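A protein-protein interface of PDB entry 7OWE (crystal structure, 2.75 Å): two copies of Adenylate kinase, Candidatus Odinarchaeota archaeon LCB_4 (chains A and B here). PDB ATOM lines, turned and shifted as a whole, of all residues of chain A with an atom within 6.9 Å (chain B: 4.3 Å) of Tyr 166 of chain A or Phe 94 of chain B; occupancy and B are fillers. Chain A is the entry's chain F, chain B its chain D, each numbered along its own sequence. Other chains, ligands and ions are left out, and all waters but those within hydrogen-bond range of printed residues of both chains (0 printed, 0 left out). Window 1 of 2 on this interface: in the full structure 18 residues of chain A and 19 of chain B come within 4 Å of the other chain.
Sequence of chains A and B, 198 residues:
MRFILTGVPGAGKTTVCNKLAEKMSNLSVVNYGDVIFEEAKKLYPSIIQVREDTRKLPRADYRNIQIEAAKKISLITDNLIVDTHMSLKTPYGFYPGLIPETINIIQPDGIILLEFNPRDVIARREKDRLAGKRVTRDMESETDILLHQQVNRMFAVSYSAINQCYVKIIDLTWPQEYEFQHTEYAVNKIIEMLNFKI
NH1 of Arg 59 of chain B is in salt-bridge range of OD1 of Asp 109 of chain A (3.4 Å). The side-chain hydroxyl of Tyr 95 of chain B is in hydrogen-bond range of the side-chain amide nitrogen of Gln 164 of chain A (2.6 Å). The side-chain hydroxyl (OH) of Tyr 166 of chain A is in hydrogen-bond range of the backbone carbonyl oxygen (O) of Leu 57 of chain B. O of Pro 108 of chain A sits at hydrogen-bond distance from NH1 of Arg 59 of chain B (3.1 Å). O of Gln 164 of chain A is in hydrogen-bond range of NE of Arg 59 of chain B (2.7 Å). N of Phe 94 of chain B is in hydrogen-bond range of O of Val 167 of chain A. The backbone carbonyl oxygen of Asn 163 of chain A is in hydrogen-bond range of the guanidinium group of Arg 59 of chain B.
The backbone carbonyl oxygen of Ile 111 of chain A lies within hydrogen-bond range of the backbone NH of Lys 168 of chain A (2.9 Å). OG1 of Thr 90 of chain B is in hydrogen-bond range of O of Gly 93 of chain B, 2.8 Å away. The backbone carbonyl oxygen (O) of Leu 88 of chain B lies within hydrogen-bond range of the backbone NH (N) of Tyr 95 of chain B, at 2.9 Å. The side-chain hydroxyl (OG1) of Thr 90 of chain B lies close to the backbone NH (N) of Tyr 92 of chain B (3.0 Å). The side-chain hydroxyl (OG) of Ser 160 of chain A lies within hydrogen-bond range of the backbone carbonyl oxygen (O) of Cys 165 of chain A (2.5 Å). The backbone carbonyl oxygen (O) of Tyr 166 of chain A is in hydrogen-bond range of the backbone NH (N) of Ile 111 of chain A (2.9 Å).
Among the printed residues, pairs that only touch across the chains: Met 193 of chain A with Tyr 92 of chain B, Val 167 of chain A with Gly 93 of chain B, Tyr 166 of chain A with Phe 94 of chain B, Tyr 166 of chain A with Tyr 92 of chain B, Lys 168 of chain A with Tyr 92 of chain B, Tyr 166 of chain A with Tyr 95 of chain B, Tyr 166 of chain A with Thr 90 of chain B, Lys 168 of chain A with Gly 93 of chain B, Tyr 166 of chain A with Arg 59 of chain B, Ile 169 of chain A with Leu 147 of chain B, Cys 165 of chain A with Phe 94 of chain B and Phe 3 of chain A with Tyr 92 of chain B.
Of chain B, only Leu 57, Arg 59, Thr 90, Tyr 92, Phe 94 and Tyr 95 come within 4 Å of Tyr 166 of chain A. Of chain A, only Cys 165, Tyr 166 and Val 167 come within 4 Å of Phe 94 of chain B. Printed residues of chain B within 4 Å of Val 167 of chain A: Gly 93 and Phe 94. Of the printed residues of chain A, Tyr 92 of chain B touches Phe 3 (3.9 Å), Tyr 166 (3.3 Å), Lys 168 (3.4 Å) and Met 193 (3.1 Å). Of the printed residues of chain A, Leu 147 of chain B touches Ile 169 (3.7 Å). Ile 112 of chain A touches none of the printed residues of chain B. Ser 87 of chain B touches none of the printed residues of chain A.
Of the 17 printed residues of chain A, 11 touch a printed residue of chain B. Printed residues of chain B that touch a printed residue of chain A: Leu 57, Arg 59, Thr 90, Tyr 92, Gly 93, Phe 94, Tyr 95 and Leu 147. Hydrophobic or aromatic side chains of chain B that line the printed part of chain A: Tyr 92, Phe 94, Tyr 95 and Leu 147. Among the printed residues, Asp or Glu carboxylates within 4 Å of a Lys or Arg side-chain nitrogen of the other chain: Asp 109 of chain A with Arg 59 of chain B (3.4 Å).
No position is printed for both chains. Of the 19 pairs that touch across the chains among the printed residues, none has its exchanged pair printed and touching as well.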
ATOM      1  N   PHE A   3      16.974  24.396   3.815  1.00  0.00           N
ATOM      2  CA  PHE A   3      17.325  23.394   4.809  1.00  0.00           C
ATOM      3  C   PHE A   3      16.358  22.224   4.738  1.00  0.00           C
ATOM      4  O   PHE A   3      15.140  22.419   4.670  1.00  0.00           O
ATOM      5  CB  PHE A   3      17.297  23.977   6.228  1.00  0.00           C
ATOM      6  CG  PHE A   3      18.441  24.889   6.533  1.00  0.00           C
ATOM      7  CD1 PHE A   3      19.725  24.389   6.661  1.00  0.00           C
ATOM      8  CD2 PHE A   3      18.234  26.245   6.711  1.00  0.00           C
ATOM      9  CE1 PHE A   3      20.784  25.226   6.947  1.00  0.00           C
ATOM     10  CE2 PHE A   3      19.287  27.086   6.999  1.00  0.00           C
ATOM     11  CZ  PHE A   3      20.565  26.576   7.117  1.00  0.00           C
ATOM     12  N   PRO A 108      20.092  21.992  -1.451  1.00  0.00           N
ATOM     13  CA  PRO A 108      19.975  22.400  -0.047  1.00  0.00           C
ATOM     14  C   PRO A 108      21.248  23.044   0.479  1.00  0.00           C
ATOM     15  O   PRO A 108      22.363  22.606   0.181  1.00  0.00           O
ATOM     16  CB  PRO A 108      19.693  21.077   0.673  1.00  0.00           C
ATOM     17  CG  PRO A 108      20.457  20.073  -0.138  1.00  0.00           C
ATOM     18  CD  PRO A 108      20.386  20.551  -1.582  1.00  0.00           C
ATOM     19  N   ASP A 109      21.068  24.098   1.279  1.00  0.00           N
ATOM     20  CA  ASP A 109      22.195  24.657   2.016  1.00  0.00           C
ATOM     21  C   ASP A 109      22.559  23.797   3.215  1.00  0.00           C
ATOM     22  O   ASP A 109      23.735  23.731   3.591  1.00  0.00           O
ATOM     23  CB  ASP A 109      21.883  26.072   2.495  1.00  0.00           C
ATOM     24  CG  ASP A 109      21.706  27.041   1.360  1.00  0.00           C
ATOM     25  OD1 ASP A 109      22.638  27.169   0.537  1.00  0.00           O
ATOM     26  OD2 ASP A 109      20.628  27.665   1.289  1.00  0.00           O
ATOM     27  N   GLY A 110      21.577  23.142   3.838  1.00  0.00           N
ATOM     28  CA  GLY A 110      21.941  22.316   4.976  1.00  0.00           C
ATOM     29  C   GLY A 110      20.913  21.267   5.327  1.00  0.00           C
ATOM     30  O   GLY A 110      19.789  21.258   4.822  1.00  0.00           O
ATOM     31  N   ILE A 111      21.336  20.368   6.217  1.00  0.00           N
ATOM     32  CA  ILE A 111      20.481  19.334   6.794  1.00  0.00           C
ATOM     33  C   ILE A 111      20.354  19.604   8.287  1.00  0.00           C
ATOM     34  O   ILE A 111      21.326  19.999   8.939  1.00  0.00           O
ATOM     35  CB  ILE A 111      21.050  17.925   6.541  1.00  0.00           C
ATOM     36  CG1 ILE A 111      21.281  17.699   5.047  1.00  0.00           C
ATOM     37  CG2 ILE A 111      20.107  16.862   7.089  1.00  0.00           C
ATOM     38  CD1 ILE A 111      22.063  16.443   4.729  1.00  0.00           C
ATOM     39  N   ILE A 112      19.158  19.387   8.825  1.00  0.00           N
ATOM     40  CA  ILE A 112      18.843  19.641  10.226  1.00  0.00           C
ATOM     41  C   ILE A 112      18.342  18.329  10.810  1.00  0.00           C
ATOM     42  O   ILE A 112      17.361  17.756  10.313  1.00  0.00           O
ATOM     43  CB  ILE A 112      17.787  20.745  10.387  1.00  0.00           C
ATOM     44  CG1 ILE A 112      18.249  22.047   9.729  1.00  0.00           C
ATOM     45  CG2 ILE A 112      17.469  20.977  11.862  1.00  0.00           C
ATOM     46  CD1 ILE A 112      17.175  23.115   9.698  1.00  0.00           C
ATOM     47  N   ALA A 156      23.913  12.207   7.048  1.00  0.00           N
ATOM     48  CA  ALA A 156      23.990  13.656   6.911  1.00  0.00           C
ATOM     49  C   ALA A 156      25.427  14.105   6.702  1.00  0.00           C
ATOM     50  O   ALA A 156      25.705  14.948   5.843  1.00  0.00           O
ATOM     51  CB  ALA A 156      23.394  14.329   8.147  1.00  0.00           C
ATOM     52  N   VAL A 157      26.356  13.541   7.474  1.00  0.00           N
ATOM     53  CA  VAL A 157      27.757  13.932   7.352  1.00  0.00           C
ATOM     54  C   VAL A 157      28.307  13.548   5.984  1.00  0.00           C
ATOM     55  O   VAL A 157      29.071  14.306   5.373  1.00  0.00           O
ATOM     56  CB  VAL A 157      28.589  13.308   8.486  1.00  0.00           C
ATOM     57  CG1 VAL A 157      30.075  13.445   8.193  1.00  0.00           C
ATOM     58  CG2 VAL A 157      28.234  13.966   9.805  1.00  0.00           C
ATOM     59  N   SER A 160      27.071  15.969   3.382  1.00  0.00           N
ATOM     60  CA  SER A 160      27.650  17.273   3.594  1.00  0.00           C
ATOM     61  C   SER A 160      29.062  17.309   3.061  1.00  0.00           C
ATOM     62  O   SER A 160      29.459  18.262   2.410  1.00  0.00           O
ATOM     63  CB  SER A 160      27.675  17.604   5.076  1.00  0.00           C
ATOM     64  OG  SER A 160      28.421  18.779   5.306  1.00  0.00           O
ATOM     65  N   ASN A 163      28.714  17.388  -0.712  1.00  0.00           N
ATOM     66  CA  ASN A 163      28.017  18.524  -1.307  1.00  0.00           C
ATOM     67  C   ASN A 163      28.228  19.844  -0.572  1.00  0.00           C
ATOM     68  O   ASN A 163      27.508  20.811  -0.850  1.00  0.00           O
ATOM     69  CB  ASN A 163      26.512  18.236  -1.393  1.00  0.00           C
ATOM     70  CG  ASN A 163      26.180  17.164  -2.406  1.00  0.00           C
ATOM     71  OD1 ASN A 163      25.695  16.092  -2.050  1.00  0.00           O
ATOM     72  ND2 ASN A 163      26.436  17.449  -3.680  1.00  0.00           N
ATOM     73  N   GLN A 164      29.183  19.921   0.351  1.00  0.00           N
ATOM     74  CA  GLN A 164      29.567  21.204   0.942  1.00  0.00           C
ATOM     75  C   GLN A 164      28.367  21.915   1.569  1.00  0.00           C
ATOM     76  O   GLN A 164      28.216  23.133   1.458  1.00  0.00           O
ATOM     77  CB  GLN A 164      30.242  22.085  -0.118  1.00  0.00           C
ATOM     78  CG  GLN A 164      30.842  23.391   0.382  1.00  0.00           C
ATOM     79  CD  GLN A 164      30.131  24.621  -0.171  1.00  0.00           C
ATOM     80  OE1 GLN A 164      29.403  24.548  -1.161  1.00  0.00           O
ATOM     81  NE2 GLN A 164      30.341  25.761   0.477  1.00  0.00           N
ATOM     82  N   CYS A 165      27.501  21.148   2.231  1.00  0.00           N
ATOM     83  CA  CYS A 165      26.343  21.690   2.932  1.00  0.00           C
ATOM     84  C   CYS A 165      26.618  21.689   4.430  1.00  0.00           C
ATOM     85  O   CYS A 165      27.623  21.156   4.907  1.00  0.00           O
ATOM     86  CB  CYS A 165      25.050  20.985   2.506  1.00  0.00           C
ATOM     87  SG  CYS A 165      24.871  19.305   3.143  1.00  0.00           S
ATOM     88  N   TYR A 166      25.689  22.282   5.176  1.00  0.00           N
ATOM     89  CA  TYR A 166      25.771  22.306   6.627  1.00  0.00           C
ATOM     90  C   TYR A 166      25.085  21.085   7.239  1.00  0.00           C
ATOM     91  O   TYR A 166      24.190  20.477   6.648  1.00  0.00           O
ATOM     92  CB  TYR A 166      25.130  23.581   7.182  1.00  0.00           C
ATOM     93  CG  TYR A 166      25.814  24.866   6.766  1.00  0.00           C
ATOM     94  CD1 TYR A 166      27.138  25.112   7.103  1.00  0.00           C
ATOM     95  CD2 TYR A 166      25.129  25.841   6.054  1.00  0.00           C
ATOM     96  CE1 TYR A 166      27.763  26.284   6.731  1.00  0.00           C
ATOM     97  CE2 TYR A 166      25.745  27.017   5.680  1.00  0.00           C
ATOM     98  CZ  TYR A 166      27.062  27.233   6.021  1.00  0.00           C
ATOM     99  OH  TYR A 166      27.682  28.405   5.651  1.00  0.00           O
ATOM    100  N   VAL A 167      25.512  20.744   8.453  1.00  0.00           N
ATOM    101  CA  VAL A 167      24.888  19.701   9.264  1.00  0.00           C
ATOM    102  C   VAL A 167      24.600  20.321  10.626  1.00  0.00           C
ATOM    103  O   VAL A 167      25.528  20.575  11.403  1.00  0.00           O
ATOM    104  CB  VAL A 167      25.776  18.456   9.410  1.00  0.00           C
ATOM    105  CG1 VAL A 167      24.980  17.293   9.984  1.00  0.00           C
ATOM    106  CG2 VAL A 167      26.385  18.072   8.074  1.00  0.00           C
ATOM    107  N   LYS A 168      23.325  20.576  10.910  1.00  0.00           N
ATOM    108  CA  LYS A 168      22.884  21.211  12.147  1.00  0.00           C
ATOM    109  C   LYS A 168      22.199  20.158  13.002  1.00  0.00           C
ATOM    110  O   LYS A 168      21.221  19.550  12.562  1.00  0.00           O
ATOM    111  CB  LYS A 168      21.921  22.365  11.856  1.00  0.00           C
ATOM    112  CG  LYS A 168      21.431  23.123  13.087  1.00  0.00           C
ATOM    113  CD  LYS A 168      22.399  24.228  13.489  1.00  0.00           C
ATOM    114  CE  LYS A 168      21.896  24.996  14.705  1.00  0.00           C
ATOM    115  NZ  LYS A 168      22.861  26.045  15.144  1.00  0.00           N
ATOM    116  N   ILE A 169      22.694  19.960  14.217  1.00  0.00           N
ATOM    117  CA  ILE A 169      22.135  18.974  15.135  1.00  0.00           C
ATOM    118  C   ILE A 169      21.459  19.719  16.274  1.00  0.00           C
ATOM    119  O   ILE A 169      22.109  20.481  16.999  1.00  0.00           O
ATOM    120  CB  ILE A 169      23.208  18.009  15.660  1.00  0.00           C
ATOM    121  CG1 ILE A 169      23.820  17.244  14.485  1.00  0.00           C
ATOM    122  CG2 ILE A 169      22.597  17.060  16.672  1.00  0.00           C
ATOM    123  CD1 ILE A 169      25.003  16.379  14.844  1.00  0.00           C
ATOM    124  N   MET A 193      18.611  30.526  12.861  1.00  0.00           N
ATOM    125  CA  MET A 193      19.415  30.195  11.691  1.00  0.00           C
ATOM    126  C   MET A 193      18.988  31.028  10.491  1.00  0.00           C
ATOM    127  O   MET A 193      19.811  31.704   9.863  1.00  0.00           O
ATOM    128  CB  MET A 193      19.288  28.708  11.362  1.00  0.00           C
ATOM    129  CG  MET A 193      19.950  27.776  12.351  1.00  0.00           C
ATOM    130  SD  MET A 193      19.628  26.056  11.917  1.00  0.00           S
ATOM    131  CE  MET A 193      20.685  25.861  10.486  1.00  0.00           C
ATOM    132  N   LEU B  57      30.702  33.045   6.805  1.00  0.00           N
ATOM    133  CA  LEU B  57      30.605  33.388   5.396  1.00  0.00           C
ATOM    134  C   LEU B  57      29.602  32.482   4.684  1.00  0.00           C
ATOM    135  O   LEU B  57      29.458  31.306   5.029  1.00  0.00           O
ATOM    136  CB  LEU B  57      31.965  33.265   4.716  1.00  0.00           C
ATOM    137  CG  LEU B  57      32.990  34.367   4.975  1.00  0.00           C
ATOM    138  CD1 LEU B  57      34.318  33.982   4.341  1.00  0.00           C
ATOM    139  CD2 LEU B  57      32.506  35.701   4.438  1.00  0.00           C
ATOM    140  N   ARG B  59      28.054  29.926   1.888  1.00  0.00           N
ATOM    141  CA  ARG B  59      28.679  28.707   1.384  1.00  0.00           C
ATOM    142  C   ARG B  59      29.526  28.976   0.148  1.00  0.00           C
ATOM    143  O   ARG B  59      30.642  28.464   0.029  1.00  0.00           O
ATOM    144  CB  ARG B  59      27.610  27.671   1.048  1.00  0.00           C
ATOM    145  CG  ARG B  59      26.897  27.047   2.221  1.00  0.00           C
ATOM    146  CD  ARG B  59      25.909  26.031   1.679  1.00  0.00           C
ATOM    147  NE  ARG B  59      26.577  25.109   0.761  1.00  0.00           N
ATOM    148  CZ  ARG B  59      25.979  24.456  -0.230  1.00  0.00           C
ATOM    149  NH1 ARG B  59      24.682  24.616  -0.451  1.00  0.00           N
ATOM    150  NH2 ARG B  59      26.684  23.644  -1.007  1.00  0.00           N
ATOM    151  N   SER B  87      35.772  19.852  10.438  1.00  0.00           N
ATOM    152  CA  SER B  87      34.501  20.555  10.340  1.00  0.00           C
ATOM    153  C   SER B  87      34.575  21.799  11.213  1.00  0.00           C
ATOM    154  O   SER B  87      35.369  21.873  12.154  1.00  0.00           O
ATOM    155  CB  SER B  87      33.324  19.667  10.760  1.00  0.00           C
ATOM    156  OG  SER B  87      33.421  19.287  12.122  1.00  0.00           O
ATOM    157  N   LEU B  88      33.738  22.777  10.882  1.00  0.00           N
ATOM    158  CA  LEU B  88      33.702  24.045  11.596  1.00  0.00           C
ATOM    159  C   LEU B  88      32.279  24.332  12.058  1.00  0.00           C
ATOM    160  O   LEU B  88      31.322  24.122  11.307  1.00  0.00           O
ATOM    161  CB  LEU B  88      34.205  25.197  10.714  1.00  0.00           C
ATOM    162  CG  LEU B  88      35.631  25.122  10.158  1.00  0.00           C
ATOM    163  CD1 LEU B  88      36.645  24.803  11.254  1.00  0.00           C
ATOM    164  CD2 LEU B  88      35.736  24.112   9.017  1.00  0.00           C
ATOM    165  N   LYS B  89      32.148  24.810  13.298  1.00  0.00           N
ATOM    166  CA  LYS B  89      30.845  25.122  13.877  1.00  0.00           C
ATOM    167  C   LYS B  89      30.422  26.513  13.419  1.00  0.00           C
ATOM    168  O   LYS B  89      31.046  27.514  13.787  1.00  0.00           O
ATOM    169  CB  LYS B  89      30.899  25.044  15.401  1.00  0.00           C
ATOM    170  CG  LYS B  89      29.552  25.254  16.094  1.00  0.00           C
ATOM    171  CD  LYS B  89      29.676  25.108  17.612  1.00  0.00           C
ATOM    172  CE  LYS B  89      28.330  25.258  18.315  1.00  0.00           C
ATOM    173  NZ  LYS B  89      28.453  25.168  19.803  1.00  0.00           N
ATOM    174  N   THR B  90      29.368  26.578  12.616  1.00  0.00           N
ATOM    175  CA  THR B  90      28.807  27.802  12.087  1.00  0.00           C
ATOM    176  C   THR B  90      27.411  28.010  12.654  1.00  0.00           C
ATOM    177  O   THR B  90      26.786  27.068  13.154  1.00  0.00           O
ATOM    178  CB  THR B  90      28.720  27.737  10.557  1.00  0.00           C
ATOM    179  OG1 THR B  90      27.574  26.965  10.178  1.00  0.00           O
ATOM    180  CG2 THR B  90      29.971  27.087   9.973  1.00  0.00           C
ATOM    181  N   TYR B  92      24.925  27.876  11.219  1.00  0.00           N
ATOM    182  CA  TYR B  92      24.078  27.003  10.417  1.00  0.00           C
ATOM    183  C   TYR B  92      24.323  25.524  10.676  1.00  0.00           C
ATOM    184  O   TYR B  92      23.632  24.688  10.085  1.00  0.00           O
ATOM    185  CB  TYR B  92      24.309  27.314   8.940  1.00  0.00           C
ATOM    186  CG  TYR B  92      23.976  28.744   8.580  1.00  0.00           C
ATOM    187  CD1 TYR B  92      22.753  29.294   8.933  1.00  0.00           C
ATOM    188  CD2 TYR B  92      24.884  29.547   7.903  1.00  0.00           C
ATOM    189  CE1 TYR B  92      22.437  30.597   8.613  1.00  0.00           C
ATOM    190  CE2 TYR B  92      24.575  30.856   7.576  1.00  0.00           C
ATOM    191  CZ  TYR B  92      23.350  31.374   7.937  1.00  0.00           C
ATOM    192  OH  TYR B  92      23.028  32.671   7.617  1.00  0.00           O
ATOM    193  N   GLY B  93      25.274  25.180  11.539  1.00  0.00           N
ATOM    194  CA  GLY B  93      25.620  23.790  11.766  1.00  0.00           C
ATOM    195  C   GLY B  93      27.084  23.524  11.486  1.00  0.00           C
ATOM    196  O   GLY B  93      27.887  24.456  11.455  1.00  0.00           O
ATOM    197  N   PHE B  94      27.455  22.269  11.279  1.00  0.00           N
ATOM    198  CA  PHE B  94      28.837  21.940  10.960  1.00  0.00           C
ATOM    199  C   PHE B  94      29.064  22.040   9.460  1.00  0.00           C
ATOM    200  O   PHE B  94      28.223  21.618   8.660  1.00  0.00           O
ATOM    201  CB  PHE B  94      29.189  20.541  11.463  1.00  0.00           C
ATOM    202  CG  PHE B  94      29.162  20.421  12.957  1.00  0.00           C
ATOM    203  CD1 PHE B  94      30.179  20.966  13.724  1.00  0.00           C
ATOM    204  CD2 PHE B  94      28.117  19.779  13.596  1.00  0.00           C
ATOM    205  CE1 PHE B  94      30.155  20.867  15.100  1.00  0.00           C
ATOM    206  CE2 PHE B  94      28.089  19.674  14.972  1.00  0.00           C
ATOM    207  CZ  PHE B  94      29.109  20.219  15.726  1.00  0.00           C
ATOM    208  N   TYR B  95      30.202  22.616   9.084  1.00  0.00           N
ATOM    209  CA  TYR B  95      30.567  22.813   7.691  1.00  0.00           C
ATOM    210  C   TYR B  95      31.853  22.056   7.395  1.00  0.00           C
ATOM    211  O   TYR B  95      32.804  22.139   8.185  1.00  0.00           O
ATOM    212  CB  TYR B  95      30.753  24.307   7.396  1.00  0.00           C
ATOM    213  CG  TYR B  95      31.185  24.610   5.982  1.00  0.00           C
ATOM    214  CD1 TYR B  95      30.261  24.677   4.950  1.00  0.00           C
ATOM    215  CD2 TYR B  95      32.520  24.844   5.681  1.00  0.00           C
ATOM    216  CE1 TYR B  95      30.652  24.960   3.658  1.00  0.00           C
ATOM    217  CE2 TYR B  95      32.921  25.128   4.394  1.00  0.00           C
ATOM    218  CZ  TYR B  95      31.986  25.187   3.385  1.00  0.00           C
ATOM    219  OH  TYR B  95      32.388  25.470   2.100  1.00  0.00           O
ATOM    220  N   LEU B 147      30.212  16.215  20.831  1.00  0.00           N
ATOM    221  CA  LEU B 147      29.523  16.165  19.546  1.00  0.00           C
ATOM    222  C   LEU B 147      30.454  16.581  18.416  1.00  0.00           C
ATOM    223  O   LEU B 147      30.551  15.898  17.388  1.00  0.00           O
ATOM    224  CB  LEU B 147      28.292  17.073  19.595  1.00  0.00           C
ATOM    225  CG  LEU B 147      27.378  17.185  18.377  1.00  0.00           C
ATOM    226  CD1 LEU B 147      26.558  15.919  18.186  1.00  0.00           C
ATOM    227  CD2 LEU B 147      26.457  18.395  18.507  1.00  0.00           C
ATOM    228  N   HIS B 148      31.137  17.715  18.591  1.00  0.00           N
ATOM    229  CA  HIS B 148      32.073  18.195  17.582  1.00  0.00           C
ATOM    230  C   HIS B 148      33.112  17.135  17.251  1.00  0.00           C
ATOM    231  O   HIS B 148      33.465  16.945  16.081  1.00  0.00           O
ATOM    232  CB  HIS B 148      32.747  19.476  18.077  1.00  0.00           C
ATOM    233  CG  HIS B 148      33.414  20.274  17.000  1.00  0.00           C
ATOM    234  ND1 HIS B 148      33.739  19.744  15.769  1.00  0.00           N
ATOM    235  CD2 HIS B 148      33.814  21.568  16.969  1.00  0.00           C
ATOM    236  CE1 HIS B 148      34.312  20.677  15.029  1.00  0.00           C
ATOM    237  NE2 HIS B 148      34.370  21.792  15.734  1.00  0.00           N
ATOM    238  N   VAL B 151      31.673  14.177  15.292  1.00  0.00           N
ATOM    239  CA  VAL B 151      31.370  14.636  13.940  1.00  0.00           C
ATOM    240  C   VAL B 151      32.650  14.788  13.122  1.00  0.00           C
ATOM    241  O   VAL B 151      32.671  14.493  11.918  1.00  0.00           O
ATOM    242  CB  VAL B 151      30.569  15.949  13.990  1.00  0.00           C
ATOM    243  CG1 VAL B 151      30.520  16.585  12.613  1.00  0.00           C
ATOM    244  CG2 VAL B 151      29.163  15.694  14.513  1.00  0.00           C
